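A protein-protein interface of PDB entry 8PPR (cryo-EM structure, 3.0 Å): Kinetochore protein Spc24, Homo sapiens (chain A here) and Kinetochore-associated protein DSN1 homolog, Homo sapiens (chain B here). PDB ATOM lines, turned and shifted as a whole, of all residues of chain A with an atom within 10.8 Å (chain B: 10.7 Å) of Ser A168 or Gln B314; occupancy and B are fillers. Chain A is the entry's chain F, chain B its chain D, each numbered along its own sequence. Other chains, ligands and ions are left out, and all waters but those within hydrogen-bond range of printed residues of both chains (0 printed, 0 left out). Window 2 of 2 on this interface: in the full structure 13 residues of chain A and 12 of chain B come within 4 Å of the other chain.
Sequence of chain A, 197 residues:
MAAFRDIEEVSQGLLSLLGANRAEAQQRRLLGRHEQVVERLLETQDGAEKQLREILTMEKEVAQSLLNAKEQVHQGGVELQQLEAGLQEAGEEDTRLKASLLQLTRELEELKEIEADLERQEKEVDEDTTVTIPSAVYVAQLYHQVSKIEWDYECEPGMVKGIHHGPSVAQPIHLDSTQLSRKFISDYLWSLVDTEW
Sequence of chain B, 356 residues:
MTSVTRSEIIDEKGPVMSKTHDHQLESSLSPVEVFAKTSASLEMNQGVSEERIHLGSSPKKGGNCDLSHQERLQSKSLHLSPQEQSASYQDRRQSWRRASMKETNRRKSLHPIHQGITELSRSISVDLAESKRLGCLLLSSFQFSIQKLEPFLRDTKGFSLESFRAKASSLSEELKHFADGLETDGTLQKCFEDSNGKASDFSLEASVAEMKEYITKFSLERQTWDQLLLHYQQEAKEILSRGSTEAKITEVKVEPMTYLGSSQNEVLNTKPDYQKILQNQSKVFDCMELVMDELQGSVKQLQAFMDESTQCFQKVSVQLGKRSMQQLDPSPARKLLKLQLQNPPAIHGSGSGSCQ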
ATOM      1  N   LYS A 148      13.726 -25.161 -10.621  1.00  0.00           N
ATOM      2  CA  LYS A 148      13.995 -25.032 -12.055  1.00  0.00           C
ATOM      3  C   LYS A 148      13.129 -26.001 -12.856  1.00  0.00           C
ATOM      4  O   LYS A 148      13.562 -26.579 -13.854  1.00  0.00           O
ATOM      5  CB  LYS A 148      15.478 -25.236 -12.367  1.00  0.00           C
ATOM      6  CG  LYS A 148      16.395 -24.266 -11.647  1.00  0.00           C
ATOM      7  CD  LYS A 148      17.848 -24.527 -11.995  1.00  0.00           C
ATOM      8  CE  LYS A 148      18.186 -23.979 -13.369  1.00  0.00           C
ATOM      9  NZ  LYS A 148      18.125 -22.491 -13.399  1.00  0.00           N
ATOM     10  N   ILE A 163       9.255 -29.835 -17.566  1.00  0.00           N
ATOM     11  CA  ILE A 163      10.606 -29.620 -18.066  1.00  0.00           C
ATOM     12  C   ILE A 163      11.522 -29.345 -16.885  1.00  0.00           C
ATOM     13  O   ILE A 163      11.216 -28.494 -16.041  1.00  0.00           O
ATOM     14  CB  ILE A 163      10.658 -28.456 -19.072  1.00  0.00           C
ATOM     15  CG1 ILE A 163       9.821 -28.783 -20.311  1.00  0.00           C
ATOM     16  CG2 ILE A 163      12.097 -28.129 -19.433  1.00  0.00           C
ATOM     17  CD1 ILE A 163       9.570 -27.593 -21.209  1.00  0.00           C
ATOM     18  N   HIS A 164      12.640 -30.060 -16.827  1.00  0.00           N
ATOM     19  CA  HIS A 164      13.638 -29.866 -15.786  1.00  0.00           C
ATOM     20  C   HIS A 164      14.830 -29.122 -16.370  1.00  0.00           C
ATOM     21  O   HIS A 164      15.467 -29.602 -17.313  1.00  0.00           O
ATOM     22  CB  HIS A 164      14.078 -31.202 -15.192  1.00  0.00           C
ATOM     23  CG  HIS A 164      14.500 -31.112 -13.760  1.00  0.00           C
ATOM     24  ND1 HIS A 164      15.356 -30.135 -13.298  1.00  0.00           N
ATOM     25  CD2 HIS A 164      14.170 -31.862 -12.683  1.00  0.00           C
ATOM     26  CE1 HIS A 164      15.545 -30.297 -12.001  1.00  0.00           C
ATOM     27  NE2 HIS A 164      14.836 -31.336 -11.602  1.00  0.00           N
ATOM     28  N   HIS A 165      15.126 -27.951 -15.809  1.00  0.00           N
ATOM     29  CA  HIS A 165      16.267 -27.149 -16.220  1.00  0.00           C
ATOM     30  C   HIS A 165      17.480 -27.365 -15.327  1.00  0.00           C
ATOM     31  O   HIS A 165      18.502 -26.697 -15.512  1.00  0.00           O
ATOM     32  CB  HIS A 165      15.884 -25.670 -16.242  1.00  0.00           C
ATOM     33  CG  HIS A 165      14.853 -25.330 -17.271  1.00  0.00           C
ATOM     34  ND1 HIS A 165      15.178 -24.848 -18.521  1.00  0.00           N
ATOM     35  CD2 HIS A 165      13.501 -25.412 -17.240  1.00  0.00           C
ATOM     36  CE1 HIS A 165      14.072 -24.642 -19.212  1.00  0.00           C
ATOM     37  NE2 HIS A 165      13.041 -24.977 -18.458  1.00  0.00           N
ATOM     38  N   GLY A 166      17.387 -28.278 -14.365  1.00  0.00           N
ATOM     39  CA  GLY A 166      18.483 -28.586 -13.478  1.00  0.00           C
ATOM     40  C   GLY A 166      19.730 -29.069 -14.194  1.00  0.00           C
ATOM     41  O   GLY A 166      20.829 -28.547 -13.980  1.00  0.00           O
ATOM     42  N   PRO A 167      19.594 -30.078 -15.053  1.00  0.00           N
ATOM     43  CA  PRO A 167      20.748 -30.530 -15.836  1.00  0.00           C
ATOM     44  C   PRO A 167      21.222 -29.457 -16.803  1.00  0.00           C
ATOM     45  O   PRO A 167      20.525 -28.482 -17.093  1.00  0.00           O
ATOM     46  CB  PRO A 167      20.212 -31.753 -16.588  1.00  0.00           C
ATOM     47  CG  PRO A 167      19.080 -32.232 -15.759  1.00  0.00           C
ATOM     48  CD  PRO A 167      18.454 -31.001 -15.187  1.00  0.00           C
ATOM     49  N   SER A 168      22.448 -29.653 -17.297  1.00  0.00           N
ATOM     50  CA  SER A 168      23.021 -28.706 -18.248  1.00  0.00           C
ATOM     51  C   SER A 168      22.176 -28.622 -19.511  1.00  0.00           C
ATOM     52  O   SER A 168      21.945 -27.530 -20.043  1.00  0.00           O
ATOM     53  CB  SER A 168      24.455 -29.108 -18.585  1.00  0.00           C
ATOM     54  OG  SER A 168      25.199 -29.362 -17.407  1.00  0.00           O
ATOM     55  N   VAL A 169      21.707 -29.763 -20.003  1.00  0.00           N
ATOM     56  CA  VAL A 169      20.767 -29.823 -21.115  1.00  0.00           C
ATOM     57  C   VAL A 169      19.400 -30.152 -20.538  1.00  0.00           C
ATOM     58  O   VAL A 169      19.230 -31.189 -19.884  1.00  0.00           O
ATOM     59  CB  VAL A 169      21.193 -30.858 -22.167  1.00  0.00           C
ATOM     60  CG1 VAL A 169      20.153 -30.947 -23.267  1.00  0.00           C
ATOM     61  CG2 VAL A 169      22.548 -30.490 -22.746  1.00  0.00           C
ATOM     62  N   ALA A 170      18.435 -29.263 -20.762  1.00  0.00           N
ATOM     63  CA  ALA A 170      17.101 -29.456 -20.214  1.00  0.00           C
ATOM     64  C   ALA A 170      16.490 -30.751 -20.734  1.00  0.00           C
ATOM     65  O   ALA A 170      16.612 -31.087 -21.915  1.00  0.00           O
ATOM     66  CB  ALA A 170      16.205 -28.270 -20.569  1.00  0.00           C
ATOM     67  N   GLN A 171      15.832 -31.479 -19.841  1.00  0.00           N
ATOM     68  CA  GLN A 171      15.230 -32.757 -20.175  1.00  0.00           C
ATOM     69  C   GLN A 171      13.771 -32.766 -19.751  1.00  0.00           C
ATOM     70  O   GLN A 171      13.395 -32.101 -18.780  1.00  0.00           O
ATOM     71  CB  GLN A 171      15.975 -33.914 -19.496  1.00  0.00           C
ATOM     72  CG  GLN A 171      15.960 -33.857 -17.984  1.00  0.00           C
ATOM     73  CD  GLN A 171      16.770 -34.971 -17.361  1.00  0.00           C
ATOM     74  OE1 GLN A 171      17.990 -34.870 -17.232  1.00  0.00           O
ATOM     75  NE2 GLN A 171      16.097 -36.047 -16.974  1.00  0.00           N
ATOM     76  N   PRO A 172      12.923 -33.505 -20.467  1.00  0.00           N
ATOM     77  CA  PRO A 172      11.483 -33.458 -20.180  1.00  0.00           C
ATOM     78  C   PRO A 172      11.126 -34.396 -19.037  1.00  0.00           C
ATOM     79  O   PRO A 172      11.502 -35.570 -19.036  1.00  0.00           O
ATOM     80  CB  PRO A 172      10.848 -33.912 -21.498  1.00  0.00           C
ATOM     81  CG  PRO A 172      11.862 -34.842 -22.081  1.00  0.00           C
ATOM     82  CD  PRO A 172      13.225 -34.369 -21.624  1.00  0.00           C
ATOM     83  N   SER A 191      17.318 -35.051  -7.420  1.00  0.00           N
ATOM     84  CA  SER A 191      18.572 -35.531  -7.987  1.00  0.00           C
ATOM     85  C   SER A 191      18.957 -34.729  -9.222  1.00  0.00           C
ATOM     86  O   SER A 191      20.131 -34.388  -9.411  1.00  0.00           O
ATOM     87  CB  SER A 191      18.458 -37.015  -8.326  1.00  0.00           C
ATOM     88  OG  SER A 191      19.438 -37.394  -9.275  1.00  0.00           O
ATOM     89  N   LEU A 192      17.980 -34.413 -10.071  1.00  0.00           N
ATOM     90  CA  LEU A 192      18.248 -33.669 -11.293  1.00  0.00           C
ATOM     91  C   LEU A 192      18.694 -32.239 -11.028  1.00  0.00           C
ATOM     92  O   LEU A 192      19.217 -31.593 -11.941  1.00  0.00           O
ATOM     93  CB  LEU A 192      17.003 -33.664 -12.177  1.00  0.00           C
ATOM     94  CG  LEU A 192      16.537 -35.020 -12.708  1.00  0.00           C
ATOM     95  CD1 LEU A 192      15.594 -34.831 -13.883  1.00  0.00           C
ATOM     96  CD2 LEU A 192      17.721 -35.888 -13.098  1.00  0.00           C
ATOM     97  N   VAL A 193      18.501 -31.735  -9.817  1.00  0.00           N
ATOM     98  CA  VAL A 193      18.917 -30.381  -9.474  1.00  0.00           C
ATOM     99  C   VAL A 193      20.427 -30.351  -9.292  1.00  0.00           C
ATOM    100  O   VAL A 193      21.015 -31.255  -8.688  1.00  0.00           O
ATOM    101  CB  VAL A 193      18.189 -29.901  -8.207  1.00  0.00           C
ATOM    102  CG1 VAL A 193      18.471 -28.427  -7.958  1.00  0.00           C
ATOM    103  CG2 VAL A 193      16.696 -30.153  -8.329  1.00  0.00           C
ATOM    104  N   ASP A 194      21.060 -29.306  -9.818  1.00  0.00           N
ATOM    105  CA  ASP A 194      22.504 -29.153  -9.705  1.00  0.00           C
ATOM    106  C   ASP A 194      22.859 -28.696  -8.296  1.00  0.00           C
ATOM    107  O   ASP A 194      22.390 -27.647  -7.840  1.00  0.00           O
ATOM    108  CB  ASP A 194      23.017 -28.156 -10.739  1.00  0.00           C
ATOM    109  CG  ASP A 194      24.367 -28.543 -11.298  1.00  0.00           C
ATOM    110  OD1 ASP A 194      25.091 -29.307 -10.626  1.00  0.00           O
ATOM    111  OD2 ASP A 194      24.706 -28.085 -12.410  1.00  0.00           O
ATOM    112  N   THR A 195      23.690 -29.477  -7.610  1.00  0.00           N
ATOM    113  CA  THR A 195      24.093 -29.158  -6.248  1.00  0.00           C
ATOM    114  C   THR A 195      25.352 -28.307  -6.179  1.00  0.00           C
ATOM    115  O   THR A 195      25.716 -27.857  -5.088  1.00  0.00           O
ATOM    116  CB  THR A 195      24.316 -30.443  -5.445  1.00  0.00           C
ATOM    117  OG1 THR A 195      24.598 -30.110  -4.080  1.00  0.00           O
ATOM    118  CG2 THR A 195      25.483 -31.229  -6.020  1.00  0.00           C
ATOM    119  N   GLU A 196      26.023 -28.077  -7.303  1.00  0.00           N
ATOM    120  CA  GLU A 196      27.236 -27.275  -7.290  1.00  0.00           C
ATOM    121  C   GLU A 196      26.905 -25.818  -6.998  1.00  0.00           C
ATOM    122  O   GLU A 196      25.893 -25.287  -7.464  1.00  0.00           O
ATOM    123  CB  GLU A 196      27.978 -27.408  -8.623  1.00  0.00           C
ATOM    124  CG  GLU A 196      27.191 -26.977  -9.856  1.00  0.00           C
ATOM    125  CD  GLU A 196      27.247 -25.482 -10.111  1.00  0.00           C
ATOM    126  OE1 GLU A 196      28.116 -24.807  -9.523  1.00  0.00           O
ATOM    127  OE2 GLU A 196      26.415 -24.983 -10.898  1.00  0.00           O
ATOM    128  N   MET B 306      30.845 -35.289 -31.639  1.00  0.00           N
ATOM    129  CA  MET B 306      29.825 -35.294 -30.592  1.00  0.00           C
ATOM    130  C   MET B 306      30.168 -34.274 -29.517  1.00  0.00           C
ATOM    131  O   MET B 306      29.276 -33.811 -28.801  1.00  0.00           O
ATOM    132  CB  MET B 306      29.564 -36.656 -29.930  1.00  0.00           C
ATOM    133  CG  MET B 306      30.577 -37.219 -28.959  1.00  0.00           C
ATOM    134  SD  MET B 306      32.153 -37.776 -29.557  1.00  0.00           S
ATOM    135  CE  MET B 306      31.622 -39.225 -30.461  1.00  0.00           C
ATOM    136  N   ASP B 307      31.450 -33.910 -29.383  1.00  0.00           N
ATOM    137  CA  ASP B 307      31.789 -32.811 -28.484  1.00  0.00           C
ATOM    138  C   ASP B 307      31.104 -31.522 -28.920  1.00  0.00           C
ATOM    139  O   ASP B 307      30.515 -30.805 -28.096  1.00  0.00           O
ATOM    140  CB  ASP B 307      33.304 -32.613 -28.443  1.00  0.00           C
ATOM    141  CG  ASP B 307      34.028 -33.771 -27.787  1.00  0.00           C
ATOM    142  OD1 ASP B 307      33.375 -34.795 -27.495  1.00  0.00           O
ATOM    143  OD2 ASP B 307      35.251 -33.656 -27.562  1.00  0.00           O
ATOM    144  N   GLU B 308      31.164 -31.222 -30.219  1.00  0.00           N
ATOM    145  CA  GLU B 308      30.475 -30.049 -30.747  1.00  0.00           C
ATOM    146  C   GLU B 308      28.974 -30.161 -30.530  1.00  0.00           C
ATOM    147  O   GLU B 308      28.307 -29.173 -30.198  1.00  0.00           O
ATOM    148  CB  GLU B 308      30.786 -29.903 -32.234  1.00  0.00           C
ATOM    149  CG  GLU B 308      32.192 -29.424 -32.537  1.00  0.00           C
ATOM    150  CD  GLU B 308      32.339 -28.943 -33.965  1.00  0.00           C
ATOM    151  OE1 GLU B 308      31.423 -29.202 -34.774  1.00  0.00           O
ATOM    152  OE2 GLU B 308      33.376 -28.323 -34.283  1.00  0.00           O
ATOM    153  N   SER B 309      28.425 -31.360 -30.730  1.00  0.00           N
ATOM    154  CA  SER B 309      26.994 -31.567 -30.530  1.00  0.00           C
ATOM    155  C   SER B 309      26.591 -31.283 -29.088  1.00  0.00           C
ATOM    156  O   SER B 309      25.573 -30.627 -28.834  1.00  0.00           O
ATOM    157  CB  SER B 309      26.620 -32.998 -30.915  1.00  0.00           C
ATOM    158  OG  SER B 309      27.174 -33.341 -32.171  1.00  0.00           O
ATOM    159  N   THR B 310      27.377 -31.779 -28.131  1.00  0.00           N
ATOM    160  CA  THR B 310      27.086 -31.535 -26.725  1.00  0.00           C
ATOM    161  C   THR B 310      27.169 -30.052 -26.402  1.00  0.00           C
ATOM    162  O   THR B 310      26.330 -29.521 -25.664  1.00  0.00           O
ATOM    163  CB  THR B 310      28.054 -32.324 -25.843  1.00  0.00           C
ATOM    164  OG1 THR B 310      27.925 -33.723 -26.124  1.00  0.00           O
ATOM    165  CG2 THR B 310      27.753 -32.079 -24.373  1.00  0.00           C
ATOM    166  N   GLN B 311      28.179 -29.368 -26.941  1.00  0.00           N
ATOM    167  CA  GLN B 311      28.295 -27.934 -26.702  1.00  0.00           C
ATOM    168  C   GLN B 311      27.085 -27.188 -27.251  1.00  0.00           C
ATOM    169  O   GLN B 311      26.551 -26.282 -26.597  1.00  0.00           O
ATOM    170  CB  GLN B 311      29.583 -27.404 -27.324  1.00  0.00           C
ATOM    171  CG  GLN B 311      30.835 -27.854 -26.598  1.00  0.00           C
ATOM    172  CD  GLN B 311      32.091 -27.250 -27.186  1.00  0.00           C
ATOM    173  OE1 GLN B 311      32.051 -26.187 -27.804  1.00  0.00           O
ATOM    174  NE2 GLN B 311      33.218 -27.927 -26.997  1.00  0.00           N
ATOM    175  N   CYS B 312      26.634 -27.564 -28.449  1.00  0.00           N
ATOM    176  CA  CYS B 312      25.451 -26.937 -29.031  1.00  0.00           C
ATOM    177  C   CYS B 312      24.220 -27.181 -28.166  1.00  0.00           C
ATOM    178  O   CYS B 312      23.427 -26.262 -27.918  1.00  0.00           O
ATOM    179  CB  CYS B 312      25.225 -27.468 -30.446  1.00  0.00           C
ATOM    180  SG  CYS B 312      23.622 -27.033 -31.156  1.00  0.00           S
ATOM    181  N   PHE B 313      24.045 -28.419 -27.700  1.00  0.00           N
ATOM    182  CA  PHE B 313      22.903 -28.732 -26.849  1.00  0.00           C
ATOM    183  C   PHE B 313      22.926 -27.903 -25.575  1.00  0.00           C
ATOM    184  O   PHE B 313      21.900 -27.352 -25.166  1.00  0.00           O
ATOM    185  CB  PHE B 313      22.886 -30.220 -26.504  1.00  0.00           C
ATOM    186  CG  PHE B 313      22.517 -31.105 -27.653  1.00  0.00           C
ATOM    187  CD1 PHE B 313      21.806 -30.604 -28.728  1.00  0.00           C
ATOM    188  CD2 PHE B 313      22.864 -32.444 -27.648  1.00  0.00           C
ATOM    189  CE1 PHE B 313      21.459 -31.420 -29.786  1.00  0.00           C
ATOM    190  CE2 PHE B 313      22.520 -33.266 -28.702  1.00  0.00           C
ATOM    191  CZ  PHE B 313      21.815 -32.753 -29.773  1.00  0.00           C
ATOM    192  N   GLN B 314      24.094 -27.800 -24.940  1.00  0.00           N
ATOM    193  CA  GLN B 314      24.196 -27.031 -23.706  1.00  0.00           C
ATOM    194  C   GLN B 314      23.903 -25.558 -23.949  1.00  0.00           C
ATOM    195  O   GLN B 314      23.220 -24.912 -23.146  1.00  0.00           O
ATOM    196  CB  GLN B 314      25.584 -27.206 -23.096  1.00  0.00           C
ATOM    197  CG  GLN B 314      25.865 -28.613 -22.614  1.00  0.00           C
ATOM    198  CD  GLN B 314      27.126 -28.697 -21.786  1.00  0.00           C
ATOM    199  OE1 GLN B 314      27.903 -27.745 -21.721  1.00  0.00           O
ATOM    200  NE2 GLN B 314      27.340 -29.841 -21.147  1.00  0.00           N
ATOM    201  N   LYS B 315      24.415 -25.008 -25.051  1.00  0.00           N
ATOM    202  CA  LYS B 315      24.173 -23.601 -25.348  1.00  0.00           C
ATOM    203  C   LYS B 315      22.691 -23.334 -25.569  1.00  0.00           C
ATOM    204  O   LYS B 315      22.135 -22.362 -25.043  1.00  0.00           O
ATOM    205  CB  LYS B 315      24.982 -23.179 -26.573  1.00  0.00           C
ATOM    206  CG  LYS B 315      24.639 -21.794 -27.077  1.00  0.00           C
ATOM    207  CD  LYS B 315      25.168 -21.584 -28.480  1.00  0.00           C
ATOM    208  CE  LYS B 315      24.475 -22.515 -29.458  1.00  0.00           C
ATOM    209  NZ  LYS B 315      23.053 -22.129 -29.669  1.00  0.00           N
ATOM    210  N   VAL B 316      22.027 -24.194 -26.344  1.00  0.00           N
ATOM    211  CA  VAL B 316      20.604 -23.977 -26.579  1.00  0.00           C
ATOM    212  C   VAL B 316      19.816 -24.169 -25.290  1.00  0.00           C
ATOM    213  O   VAL B 316      18.832 -23.460 -25.043  1.00  0.00           O
ATOM    214  CB  VAL B 316      20.092 -24.893 -27.704  1.00  0.00           C
ATOM    215  CG1 VAL B 316      18.622 -24.625 -27.973  1.00  0.00           C
ATOM    216  CG2 VAL B 316      20.904 -24.676 -28.967  1.00  0.00           C
ATOM    217  N   SER B 317      20.236 -25.111 -24.443  1.00  0.00           N
ATOM    218  CA  SER B 317      19.545 -25.329 -23.177  1.00  0.00           C
ATOM    219  C   SER B 317      19.651 -24.110 -22.270  1.00  0.00           C
ATOM    220  O   SER B 317      18.657 -23.696 -21.665  1.00  0.00           O
ATOM    221  CB  SER B 317      20.109 -26.565 -22.483  1.00  0.00           C
ATOM    222  OG  SER B 317      19.466 -26.790 -21.242  1.00  0.00           O
ATOM    223  N   VAL B 318      20.844 -23.523 -22.163  1.00  0.00           N
ATOM    224  CA  VAL B 318      20.982 -22.347 -21.312  1.00  0.00           C
ATOM    225  C   VAL B 318      20.253 -21.154 -21.917  1.00  0.00           C
ATOM    226  O   VAL B 318      19.708 -20.319 -21.184  1.00  0.00           O
ATOM    227  CB  VAL B 318      22.466 -22.036 -21.028  1.00  0.00           C
ATOM    228  CG1 VAL B 318      23.150 -23.250 -20.420  1.00  0.00           C
ATOM    229  CG2 VAL B 318      23.190 -21.586 -22.282  1.00  0.00           C
ATOM    230  N   GLN B 319      20.209 -21.051 -23.250  1.00  0.00           N
ATOM    231  CA  GLN B 319      19.416 -19.993 -23.866  1.00  0.00           C
ATOM    232  C   GLN B 319      17.939 -20.143 -23.528  1.00  0.00           C
ATOM    233  O   GLN B 319      17.267 -19.160 -23.190  1.00  0.00           O
ATOM    234  CB  GLN B 319      19.605 -19.996 -25.379  1.00  0.00           C
ATOM    235  CG  GLN B 319      18.722 -18.980 -26.074  1.00  0.00           C
ATOM    236  CD  GLN B 319      18.838 -19.029 -27.577  1.00  0.00           C
ATOM    237  OE1 GLN B 319      18.172 -18.273 -28.281  1.00  0.00           O
ATOM    238  NE2 GLN B 319      19.683 -19.920 -28.080  1.00  0.00           N
ATOM    239  N   LEU B 320      17.416 -21.365 -23.625  1.00  0.00           N
ATOM    240  CA  LEU B 320      16.019 -21.603 -23.281  1.00  0.00           C
ATOM    241  C   LEU B 320      15.762 -21.309 -21.811  1.00  0.00           C
ATOM    242  O   LEU B 320      14.724 -20.737 -21.453  1.00  0.00           O
ATOM    243  CB  LEU B 320      15.641 -23.043 -23.616  1.00  0.00           C
ATOM    244  CG  LEU B 320      14.173 -23.405 -23.411  1.00  0.00           C
ATOM    245  CD1 LEU B 320      13.299 -22.582 -24.340  1.00  0.00           C
ATOM    246  CD2 LEU B 320      13.964 -24.891 -23.644  1.00  0.00           C
ATOM    247  N   GLY B 321      16.699 -21.698 -20.946  1.00  0.00           N
ATOM    248  CA  GLY B 321      16.562 -21.385 -19.536  1.00  0.00           C
ATOM    249  C   GLY B 321      16.497 -19.893 -19.283  1.00  0.00           C
ATOM    250  O   GLY B 321      15.654 -19.425 -18.521  1.00  0.00           O
ATOM    251  N   LYS B 322      17.377 -19.125 -19.930  1.00  0.00           N
ATOM    252  CA  LYS B 322      17.356 -17.674 -19.771  1.00  0.00           C
ATOM    253  C   LYS B 322      16.057 -17.078 -20.295  1.00  0.00           C
ATOM    254  O   LYS B 322      15.502 -16.144 -19.698  1.00  0.00           O
ATOM    255  CB  LYS B 322      18.552 -17.054 -20.490  1.00  0.00           C
ATOM    256  CG  LYS B 322      18.705 -15.563 -20.260  1.00  0.00           C
ATOM    257  CD  LYS B 322      19.900 -15.019 -21.019  1.00  0.00           C
ATOM    258  CE  LYS B 322      21.204 -15.527 -20.426  1.00  0.00           C
ATOM    259  NZ  LYS B 322      21.436 -15.003 -19.053  1.00  0.00           N
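Gly B321 touches His A165 (CA to ND1, 3.9 Å).
NE2 of Gln B314 touches CB of Ser A168 (3.9 Å).
CG2 of Val A169 touches CB of Phe B313 (3.8 Å).
N of Gln B314 touches CG2 of Val A169, 3.8 Å away.
Val A169 touches Ser B317 (CA to OG, 3.3 Å).
The backbone carbonyl oxygen (O) of Ser A168 lies within hydrogen-bond range of the side-chain hydroxyl (OG) of Ser B317, 2.9 Å away.
The backbone NH (N) of Ala A170 is in hydrogen-bond range of the side-chain hydroxyl (OG) of Ser B317, at 2.7 Å.
Ser A168 touches just these residues of chain B: Gln B314 and Ser B317.
No residue of chain B comes within 4 Å of Pro A167.
Ala A170 touches just one residue of chain B: Ser B317.
No residue of chain A comes within 4 Å of Thr B310.
No residue of chain A comes within 4 Å of Lys B315.
Ser B317 touches just these residues of chain A: Ser A168, Val A169 and Ala A170.
No residue of chain A comes within 4 Å of Val B318.
Of the printed residues of chain A, Gly B321 touches His A165.
Of the printed residues of chain B, His A165 touches Gly B321 (3.9 Å).
The nearest residue of chain B that does not touch Ser A168 is Val B318 (4.5 Å).
O of Lys A148 sits at hydrogen-bond distance from N of His A165 (2.9 Å).
Of the 17 printed residues of chain B, 4 touch a printed residue of chain A.
Printed residues of chain B that touch a printed residue of chain A: Phe B313, Gln B314, Ser B317 and Gly B321.
Hydrophobic or aromatic side chains of chain B within 4 Å of the printed part of chain A: Phe B313.
Hydrophobic or aromatic side chains of chain A within 4 Å of the printed part of chain B: His A165, Val A169 and Ala A170.
Among the printed residues, 7 pairs touch across the chains.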
